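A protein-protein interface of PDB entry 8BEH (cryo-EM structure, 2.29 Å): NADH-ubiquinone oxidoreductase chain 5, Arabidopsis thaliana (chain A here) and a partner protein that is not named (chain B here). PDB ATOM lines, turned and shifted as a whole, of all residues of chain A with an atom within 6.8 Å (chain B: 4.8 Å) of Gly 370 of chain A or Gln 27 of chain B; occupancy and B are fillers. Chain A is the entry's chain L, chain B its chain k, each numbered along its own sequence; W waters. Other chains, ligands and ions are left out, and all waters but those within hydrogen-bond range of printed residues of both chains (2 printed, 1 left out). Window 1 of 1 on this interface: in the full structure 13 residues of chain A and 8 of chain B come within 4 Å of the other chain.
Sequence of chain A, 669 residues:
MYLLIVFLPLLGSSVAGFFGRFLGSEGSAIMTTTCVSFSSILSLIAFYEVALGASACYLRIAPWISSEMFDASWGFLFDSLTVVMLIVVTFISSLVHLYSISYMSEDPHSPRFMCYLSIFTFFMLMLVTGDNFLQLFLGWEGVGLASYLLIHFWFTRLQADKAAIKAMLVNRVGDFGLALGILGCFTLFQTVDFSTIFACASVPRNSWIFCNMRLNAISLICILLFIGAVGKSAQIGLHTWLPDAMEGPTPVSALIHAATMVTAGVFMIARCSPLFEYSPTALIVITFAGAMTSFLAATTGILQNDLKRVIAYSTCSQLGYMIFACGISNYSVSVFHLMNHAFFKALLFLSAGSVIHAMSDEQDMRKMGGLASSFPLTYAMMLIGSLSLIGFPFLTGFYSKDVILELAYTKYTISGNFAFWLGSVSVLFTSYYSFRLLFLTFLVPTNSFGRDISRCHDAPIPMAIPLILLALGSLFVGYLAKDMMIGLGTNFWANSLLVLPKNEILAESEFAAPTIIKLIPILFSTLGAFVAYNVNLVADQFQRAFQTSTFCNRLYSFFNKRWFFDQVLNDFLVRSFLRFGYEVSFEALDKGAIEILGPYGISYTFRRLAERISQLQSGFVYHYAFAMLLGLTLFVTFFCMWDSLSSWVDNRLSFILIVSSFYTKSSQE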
ATOM      1  N   MET A 368      -8.908 -10.884  29.896  1.00  0.00           N
ATOM      2  CA  MET A 368      -9.588 -11.102  28.628  1.00  0.00           C
ATOM      3  C   MET A 368      -8.593 -10.739  27.531  1.00  0.00           C
ATOM      4  O   MET A 368      -7.378 -10.710  27.753  1.00  0.00           O
ATOM      5  CB  MET A 368     -10.892 -10.288  28.568  1.00  0.00           C
ATOM      6  CG  MET A 368     -12.102 -10.989  29.172  1.00  0.00           C
ATOM      7  SD  MET A 368     -13.535  -9.903  29.334  1.00  0.00           S
ATOM      8  CE  MET A 368     -14.209 -10.424  30.913  1.00  0.00           C
ATOM      9  N   GLY A 369      -9.088 -10.490  26.333  1.00  0.00           N
ATOM     10  CA  GLY A 369      -8.212 -10.021  25.280  1.00  0.00           C
ATOM     11  C   GLY A 369      -7.927 -11.097  24.256  1.00  0.00           C
ATOM     12  O   GLY A 369      -7.973 -12.296  24.543  1.00  0.00           O
ATOM     13  N   GLY A 370      -7.632 -10.663  23.035  1.00  0.00           N
ATOM     14  CA  GLY A 370      -7.412 -11.597  21.942  1.00  0.00           C
ATOM     15  C   GLY A 370      -8.616 -12.465  21.659  1.00  0.00           C
ATOM     16  O   GLY A 370      -8.467 -13.650  21.342  1.00  0.00           O
ATOM     17  N   LEU A 371      -9.813 -11.899  21.768  1.00  0.00           N
ATOM     18  CA  LEU A 371     -11.052 -12.651  21.664  1.00  0.00           C
ATOM     19  C   LEU A 371     -11.829 -12.350  20.388  1.00  0.00           C
ATOM     20  O   LEU A 371     -12.876 -12.962  20.160  1.00  0.00           O
ATOM     21  CB  LEU A 371     -11.924 -12.361  22.891  1.00  0.00           C
ATOM     22  CG  LEU A 371     -11.995 -13.408  24.001  1.00  0.00           C
ATOM     23  CD1 LEU A 371     -10.625 -13.954  24.358  1.00  0.00           C
ATOM     24  CD2 LEU A 371     -12.665 -12.814  25.235  1.00  0.00           C
ATOM     25  N   ALA A 372     -11.345 -11.430  19.551  1.00  0.00           N
ATOM     26  CA  ALA A 372     -12.085 -11.051  18.350  1.00  0.00           C
ATOM     27  C   ALA A 372     -12.277 -12.237  17.411  1.00  0.00           C
ATOM     28  O   ALA A 372     -13.367 -12.434  16.865  1.00  0.00           O
ATOM     29  CB  ALA A 372     -11.366  -9.909  17.632  1.00  0.00           C
ATOM     30  N   SER A 373     -11.232 -13.041  17.217  1.00  0.00           N
ATOM     31  CA  SER A 373     -11.320 -14.173  16.301  1.00  0.00           C
ATOM     32  C   SER A 373     -12.099 -15.342  16.887  1.00  0.00           C
ATOM     33  O   SER A 373     -12.711 -16.106  16.135  1.00  0.00           O
ATOM     34  CB  SER A 373      -9.920 -14.628  15.897  1.00  0.00           C
ATOM     35  OG  SER A 373      -9.248 -13.590  15.213  1.00  0.00           O
ATOM     36  N   SER A 374     -12.076 -15.509  18.211  1.00  0.00           N
ATOM     37  CA  SER A 374     -12.775 -16.625  18.837  1.00  0.00           C
ATOM     38  C   SER A 374     -14.281 -16.404  18.899  1.00  0.00           C
ATOM     39  O   SER A 374     -15.046 -17.365  18.783  1.00  0.00           O
ATOM     40  CB  SER A 374     -12.219 -16.874  20.242  1.00  0.00           C
ATOM     41  OG  SER A 374     -13.002 -16.227  21.227  1.00  0.00           O
ATOM     42  N   TYR A 379     -18.157 -10.122  19.031  1.00  0.00           N
ATOM     43  CA  TYR A 379     -17.312  -8.937  18.763  1.00  0.00           C
ATOM     44  C   TYR A 379     -18.014  -7.943  17.792  1.00  0.00           C
ATOM     45  O   TYR A 379     -17.992  -6.769  18.075  1.00  0.00           O
ATOM     46  CB  TYR A 379     -15.934  -9.276  18.193  1.00  0.00           C
ATOM     47  CG  TYR A 379     -15.168  -8.048  17.769  1.00  0.00           C
ATOM     48  CD1 TYR A 379     -14.787  -7.103  18.704  1.00  0.00           C
ATOM     49  CD2 TYR A 379     -14.886  -7.790  16.441  1.00  0.00           C
ATOM     50  CE1 TYR A 379     -14.114  -5.953  18.346  1.00  0.00           C
ATOM     51  CE2 TYR A 379     -14.212  -6.644  16.060  1.00  0.00           C
ATOM     52  CZ  TYR A 379     -13.823  -5.726  17.016  1.00  0.00           C
ATOM     53  OH  TYR A 379     -13.172  -4.591  16.662  1.00  0.00           O
ATOM     54  N   PHE A 439     -10.976  -2.595  23.203  1.00  0.00           N
ATOM     55  CA  PHE A 439      -9.570  -2.954  23.069  1.00  0.00           C
ATOM     56  C   PHE A 439      -9.163  -3.996  24.105  1.00  0.00           C
ATOM     57  O   PHE A 439      -8.533  -5.004  23.768  1.00  0.00           O
ATOM     58  CB  PHE A 439      -8.719  -1.695  23.203  1.00  0.00           C
ATOM     59  CG  PHE A 439      -8.776  -0.795  22.005  1.00  0.00           C
ATOM     60  CD1 PHE A 439      -9.477  -1.167  20.871  1.00  0.00           C
ATOM     61  CD2 PHE A 439      -8.193   0.456  22.039  1.00  0.00           C
ATOM     62  CE1 PHE A 439      -9.545  -0.336  19.777  1.00  0.00           C
ATOM     63  CE2 PHE A 439      -8.265   1.295  20.947  1.00  0.00           C
ATOM     64  CZ  PHE A 439      -8.939   0.899  19.815  1.00  0.00           C
ATOM     65  N   LEU A 440      -9.516  -3.772  25.375  1.00  0.00           N
ATOM     66  CA  LEU A 440      -9.152  -4.719  26.423  1.00  0.00           C
ATOM     67  C   LEU A 440      -9.839  -6.060  26.238  1.00  0.00           C
ATOM     68  O   LEU A 440      -9.240  -7.100  26.523  1.00  0.00           O
ATOM     69  CB  LEU A 440      -9.487  -4.156  27.805  1.00  0.00           C
ATOM     70  CG  LEU A 440      -8.609  -3.026  28.335  1.00  0.00           C
ATOM     71  CD1 LEU A 440      -9.068  -2.595  29.720  1.00  0.00           C
ATOM     72  CD2 LEU A 440      -7.151  -3.437  28.345  1.00  0.00           C
ATOM     73  N   THR A 441     -11.087  -6.065  25.770  1.00  0.00           N
ATOM     74  CA  THR A 441     -11.819  -7.318  25.670  1.00  0.00           C
ATOM     75  C   THR A 441     -11.412  -8.135  24.448  1.00  0.00           C
ATOM     76  O   THR A 441     -11.311  -9.363  24.536  1.00  0.00           O
ATOM     77  CB  THR A 441     -13.322  -7.036  25.647  1.00  0.00           C
ATOM     78  OG1 THR A 441     -13.653  -6.126  26.702  1.00  0.00           O
ATOM     79  CG2 THR A 441     -14.115  -8.312  25.804  1.00  0.00           C
ATOM     80  N   PHE A 442     -11.175  -7.497  23.304  1.00  0.00           N
ATOM     81  CA  PHE A 442     -11.081  -8.265  22.069  1.00  0.00           C
ATOM     82  C   PHE A 442      -9.765  -8.134  21.318  1.00  0.00           C
ATOM     83  O   PHE A 442      -9.408  -9.059  20.588  1.00  0.00           O
ATOM     84  CB  PHE A 442     -12.221  -7.877  21.118  1.00  0.00           C
ATOM     85  CG  PHE A 442     -13.586  -8.205  21.641  1.00  0.00           C
ATOM     86  CD1 PHE A 442     -14.088  -9.492  21.548  1.00  0.00           C
ATOM     87  CD2 PHE A 442     -14.377  -7.228  22.218  1.00  0.00           C
ATOM     88  CE1 PHE A 442     -15.345  -9.792  22.020  1.00  0.00           C
ATOM     89  CE2 PHE A 442     -15.635  -7.529  22.693  1.00  0.00           C
ATOM     90  CZ  PHE A 442     -16.117  -8.811  22.594  1.00  0.00           C
ATOM     91  N   LEU A 443      -9.037  -7.032  21.465  1.00  0.00           N
ATOM     92  CA  LEU A 443      -7.963  -6.723  20.530  1.00  0.00           C
ATOM     93  C   LEU A 443      -6.556  -6.813  21.101  1.00  0.00           C
ATOM     94  O   LEU A 443      -5.626  -7.083  20.341  1.00  0.00           O
ATOM     95  CB  LEU A 443      -8.175  -5.324  19.934  1.00  0.00           C
ATOM     96  CG  LEU A 443      -9.560  -5.164  19.308  1.00  0.00           C
ATOM     97  CD1 LEU A 443      -9.736  -3.812  18.650  1.00  0.00           C
ATOM     98  CD2 LEU A 443      -9.797  -6.280  18.304  1.00  0.00           C
ATOM     99  N   VAL A 444      -6.363  -6.604  22.400  1.00  0.00           N
ATOM    100  CA  VAL A 444      -5.021  -6.649  22.979  1.00  0.00           C
ATOM    101  C   VAL A 444      -4.538  -8.095  22.997  1.00  0.00           C
ATOM    102  O   VAL A 444      -5.362  -9.016  22.929  1.00  0.00           O
ATOM    103  CB  VAL A 444      -4.987  -6.034  24.389  1.00  0.00           C
ATOM    104  CG1 VAL A 444      -5.192  -4.526  24.322  1.00  0.00           C
ATOM    105  CG2 VAL A 444      -6.010  -6.698  25.309  1.00  0.00           C
ATOM    106  N   PRO A 445      -3.230  -8.346  23.050  1.00  0.00           N
ATOM    107  CA  PRO A 445      -2.758  -9.719  23.273  1.00  0.00           C
ATOM    108  C   PRO A 445      -3.356 -10.272  24.558  1.00  0.00           C
ATOM    109  O   PRO A 445      -3.444  -9.575  25.568  1.00  0.00           O
ATOM    110  CB  PRO A 445      -1.237  -9.566  23.381  1.00  0.00           C
ATOM    111  CG  PRO A 445      -0.912  -8.229  22.865  1.00  0.00           C
ATOM    112  CD  PRO A 445      -2.154  -7.439  22.628  1.00  0.00           C
ATOM    113  N   THR A 446      -3.765 -11.538  24.509  1.00  0.00           N
ATOM    114  CA  THR A 446      -4.664 -12.074  25.522  1.00  0.00           C
ATOM    115  C   THR A 446      -4.025 -12.070  26.909  1.00  0.00           C
ATOM    116  O   THR A 446      -2.856 -12.426  27.085  1.00  0.00           O
ATOM    117  CB  THR A 446      -5.112 -13.491  25.149  1.00  0.00           C
ATOM    118  OG1 THR A 446      -6.039 -13.975  26.129  1.00  0.00           O
ATOM    119  CG2 THR A 446      -3.933 -14.446  25.066  1.00  0.00           C
ATOM    120  N   ASN A 447      -4.811 -11.644  27.894  1.00  0.00           N
ATOM    121  CA  ASN A 447      -4.420 -11.663  29.296  1.00  0.00           C
ATOM    122  C   ASN A 447      -5.236 -12.676  30.086  1.00  0.00           C
ATOM    123  O   ASN A 447      -5.293 -12.604  31.317  1.00  0.00           O
ATOM    124  CB  ASN A 447      -4.573 -10.273  29.911  1.00  0.00           C
ATOM    125  CG  ASN A 447      -3.527  -9.301  29.427  1.00  0.00           C
ATOM    126  OD1 ASN A 447      -2.337  -9.610  29.395  1.00  0.00           O
ATOM    127  ND2 ASN A 447      -3.967  -8.108  29.054  1.00  0.00           N
ATOM    128  N   ILE A 453      -9.954 -20.074  27.673  1.00  0.00           N
ATOM    129  CA  ILE A 453      -9.851 -20.055  26.176  1.00  0.00           C
ATOM    130  C   ILE A 453     -10.240 -21.407  25.614  1.00  0.00           C
ATOM    131  O   ILE A 453     -11.016 -21.446  24.699  1.00  0.00           O
ATOM    132  CB  ILE A 453      -8.385 -19.660  25.879  1.00  0.00           C
ATOM    133  CG1 ILE A 453      -8.175 -18.152  25.993  1.00  0.00           C
ATOM    134  CG2 ILE A 453      -7.923 -20.189  24.533  1.00  0.00           C
ATOM    135  CD1 ILE A 453      -9.236 -17.350  25.290  1.00  0.00           C
ATOM    136  N   MET B  23      -4.208 -17.877  16.506  1.00  0.00           N
ATOM    137  CA  MET B  23      -5.496 -17.204  16.424  1.00  0.00           C
ATOM    138  C   MET B  23      -5.912 -16.568  17.743  1.00  0.00           C
ATOM    139  O   MET B  23      -7.076 -16.192  17.906  1.00  0.00           O
ATOM    140  CB  MET B  23      -6.572 -18.159  15.906  1.00  0.00           C
ATOM    141  CG  MET B  23      -6.704 -19.494  16.593  1.00  0.00           C
ATOM    142  SD  MET B  23      -7.838 -20.482  15.589  1.00  0.00           S
ATOM    143  CE  MET B  23      -8.858 -21.282  16.816  1.00  0.00           C
ATOM    144  N   LEU B  24      -4.978 -16.431  18.679  1.00  0.00           N
ATOM    145  CA  LEU B  24      -5.155 -15.586  19.848  1.00  0.00           C
ATOM    146  C   LEU B  24      -4.388 -14.279  19.736  1.00  0.00           C
ATOM    147  O   LEU B  24      -4.574 -13.394  20.578  1.00  0.00           O
ATOM    148  CB  LEU B  24      -4.702 -16.330  21.112  1.00  0.00           C
ATOM    149  CG  LEU B  24      -5.612 -17.447  21.625  1.00  0.00           C
ATOM    150  CD1 LEU B  24      -5.415 -17.649  23.114  1.00  0.00           C
ATOM    151  CD2 LEU B  24      -7.072 -17.158  21.301  1.00  0.00           C
ATOM    152  N   SER B  25      -3.543 -14.137  18.724  1.00  0.00           N
ATOM    153  CA  SER B  25      -2.637 -13.009  18.581  1.00  0.00           C
ATOM    154  C   SER B  25      -2.921 -12.254  17.291  1.00  0.00           C
ATOM    155  O   SER B  25      -3.607 -12.744  16.391  1.00  0.00           O
ATOM    156  CB  SER B  25      -1.183 -13.485  18.599  1.00  0.00           C
ATOM    157  OG  SER B  25      -0.987 -14.517  17.652  1.00  0.00           O
ATOM    158  N   ASN B  26      -2.355 -11.047  17.211  1.00  0.00           N
ATOM    159  CA  ASN B  26      -2.496 -10.173  16.046  1.00  0.00           C
ATOM    160  C   ASN B  26      -3.968  -9.915  15.731  1.00  0.00           C
ATOM    161  O   ASN B  26      -4.392  -9.903  14.574  1.00  0.00           O
ATOM    162  CB  ASN B  26      -1.763 -10.754  14.834  1.00  0.00           C
ATOM    163  CG  ASN B  26      -0.255 -10.683  14.977  1.00  0.00           C
ATOM    164  OD1 ASN B  26       0.271  -9.864  15.731  1.00  0.00           O
ATOM    165  ND2 ASN B  26       0.449 -11.542  14.248  1.00  0.00           N
ATOM    166  N   GLN B  27      -4.752  -9.700  16.786  1.00  0.00           N
ATOM    167  CA  GLN B  27      -6.185  -9.500  16.638  1.00  0.00           C
ATOM    168  C   GLN B  27      -6.549  -8.108  16.138  1.00  0.00           C
ATOM    169  O   GLN B  27      -7.710  -7.884  15.786  1.00  0.00           O
ATOM    170  CB  GLN B  27      -6.890  -9.778  17.968  1.00  0.00           C
ATOM    171  CG  GLN B  27      -6.773 -11.218  18.415  1.00  0.00           C
ATOM    172  CD  GLN B  27      -7.429 -12.165  17.441  1.00  0.00           C
ATOM    173  OE1 GLN B  27      -8.563 -11.948  17.023  1.00  0.00           O
ATOM    174  NE2 GLN B  27      -6.715 -13.211  17.056  1.00  0.00           N
ATOM    175  N   MET B  28      -5.594  -7.179  16.083  1.00  0.00           N
ATOM    176  CA  MET B  28      -5.891  -5.853  15.552  1.00  0.00           C
ATOM    177  C   MET B  28      -6.198  -5.905  14.063  1.00  0.00           C
ATOM    178  O   MET B  28      -6.860  -5.005  13.536  1.00  0.00           O
ATOM    179  CB  MET B  28      -4.729  -4.904  15.825  1.00  0.00           C
ATOM    180  CG  MET B  28      -4.773  -4.270  17.205  1.00  0.00           C
ATOM    181  SD  MET B  28      -6.228  -3.239  17.464  1.00  0.00           S
ATOM    182  CE  MET B  28      -5.751  -1.759  16.582  1.00  0.00           C
ATOM    183  N   ARG B  29      -5.746  -6.951  13.374  1.00  0.00           N
ATOM    184  CA  ARG B  29      -6.115  -7.134  11.980  1.00  0.00           C
ATOM    185  C   ARG B  29      -7.561  -7.585  11.811  1.00  0.00           C
ATOM    186  O   ARG B  29      -8.078  -7.535  10.690  1.00  0.00           O
ATOM    187  CB  ARG B  29      -5.163  -8.129  11.315  1.00  0.00           C
ATOM    188  CG  ARG B  29      -3.735  -7.650  11.171  1.00  0.00           C
ATOM    189  CD  ARG B  29      -2.879  -8.681  10.459  1.00  0.00           C
ATOM    190  NE  ARG B  29      -1.484  -8.260  10.376  1.00  0.00           N
ATOM    191  CZ  ARG B  29      -0.493  -9.010   9.911  1.00  0.00           C
ATOM    192  NH1 ARG B  29      -0.701 -10.246   9.485  1.00  0.00           N
ATOM    193  NH2 ARG B  29       0.737  -8.507   9.872  1.00  0.00           N
ATOM    194  N   HIS B  30      -8.231  -8.013  12.872  1.00  0.00           N
ATOM    195  CA  HIS B  30      -9.642  -8.464  12.841  1.00  0.00           C
ATOM    196  C   HIS B  30     -10.588  -7.408  13.372  1.00  0.00           C
ATOM    197  O   HIS B  30     -11.743  -7.727  13.539  1.00  0.00           O
ATOM    198  CB  HIS B  30      -9.748  -9.693  13.728  1.00  0.00           C
ATOM    199  CG  HIS B  30      -9.349 -10.939  13.025  1.00  0.00           C
ATOM    200  ND1 HIS B  30      -8.036 -11.329  12.913  1.00  0.00           N
ATOM    201  CD2 HIS B  30     -10.082 -11.851  12.360  1.00  0.00           C
ATOM    202  CE1 HIS B  30      -7.978 -12.448  12.236  1.00  0.00           C
ATOM    203  NE2 HIS B  30      -9.217 -12.793  11.889  1.00  0.00           N
ATOM    204  N   ALA B  31     -10.105  -6.219  13.647  1.00  0.00           N
ATOM    205  CA  ALA B  31     -10.867  -5.169  14.330  1.00  0.00           C
ATOM    206  C   ALA B  31     -11.994  -4.536  13.485  1.00  0.00           C
ATOM    207  O   ALA B  31     -12.871  -4.005  14.064  1.00  0.00           O
ATOM    208  CB  ALA B  31      -9.840  -4.183  14.756  1.00  0.00           C
HETATM  209  O   HOH W   1      -2.205 -13.535  22.545  1.00  0.00           O
HETATM  210  O   HOH W   2     -13.445 -10.213  14.321  1.00  0.00           O
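A ring nitrogen (NE2) of His 30 of chain B sits at hydrogen-bond distance from the side-chain hydroxyl of Ser 373 of chain A (3.4 Å). The side-chain hydroxyl (OG) of Ser 373 of chain A is in hydrogen-bond range of the side-chain amide oxygen (OE1) of Gln 27 of chain B, at 2.5 Å. OH of Tyr 379 of chain A lies within hydrogen-bond range of O of Ala 31 of chain B, at 2.7 Å.
N of Gly 370 of chain A sits at hydrogen-bond distance from O of Val 444 of chain A, 2.8 Å away. N of Ala 372 of chain A sits at hydrogen-bond distance from O of Phe 442 of chain A (3.2 Å). O of Phe 442 of chain A sits at hydrogen-bond distance from N of Leu 371 of chain A. N of Gly 370 of chain A sits at hydrogen-bond distance from O of Phe 442 of chain A (3.4 Å). The side-chain amide nitrogen of Gln 27 of chain B is in hydrogen-bond range of the backbone carbonyl oxygen of Ser 25 of chain B (3.2 Å). The side-chain amide nitrogen (NE2) of Gln 27 of chain B is in hydrogen-bond range of the backbone carbonyl oxygen (O) of Met 23 of chain B (3.1 Å).
Among the printed residues, pairs that only touch across the chains: Gly 370 of chain A with Leu 24 of chain B (3.6 Å), Gly 370 of chain A with Gln 27 of chain B (3.6 Å), Ala 372 of chain A with Gln 27 of chain B (3.5 Å), Ser 373 of chain A with Met 23 of chain B (3.8 Å), Tyr 379 of chain A with His 30 of chain B (3.7 Å), Phe 442 of chain A with Gln 27 of chain B (3.7 Å), Leu 443 of chain A with Gln 27 of chain B (3.6 Å), Leu 443 of chain A with Met 28 of chain B (3.7 Å), Leu 443 of chain A with Ala 31 of chain B (3.9 Å) and Ile 453 of chain A with Leu 24 of chain B (3.8 Å).
Gln 27 of chain B touches just these residues of chain A: Gly 370 (3.6 Å), Ala 372 (3.5 Å), Ser 373 (2.5 Å), Phe 442 (3.7 Å) and Leu 443 (3.6 Å). Of the printed residues of chain B, Phe 442 of chain A touches Gln 27. Of the printed residues of chain A, Met 28 of chain B touches Leu 443 (3.7 Å). The nearest residue of chain B that does not touch Gly 370 of chain A is Met 23 of chain B (4.5 Å). The nearest residue of chain A that does not touch Gln 27 of chain B is Leu 371 of chain A (4.6 Å).
Of the 9 printed residues of chain B, 6 touch a printed residue of chain A. Hydrophobic or aromatic side chains of chain B within 4 Å of the printed part of chain A: Leu 24, Met 28, His 30 and Ala 31. Hydrophobic or aromatic side chains of chain A within 4 Å of the printed part of chain B: Ala 372, Tyr 379, Leu 443 and Ile 453. Among the printed residues, 13 pairs touch across the chains. Among the printed residues, no Asp or Glu carboxylate lies within 4 Å of a Lys or Arg side-chain nitrogen of the other chain.
Water W1 bridges the backbone carbonyl oxygen (O) of Leu 24 of chain B (3.1 Å) and the backbone NH (N) of Thr 446 of chain A (3.2 Å). Water W2 lies within hydrogen-bond range of O of His 30 of chain B (3.1 Å) and O of Ala 372 of chain A (3.4 Å).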
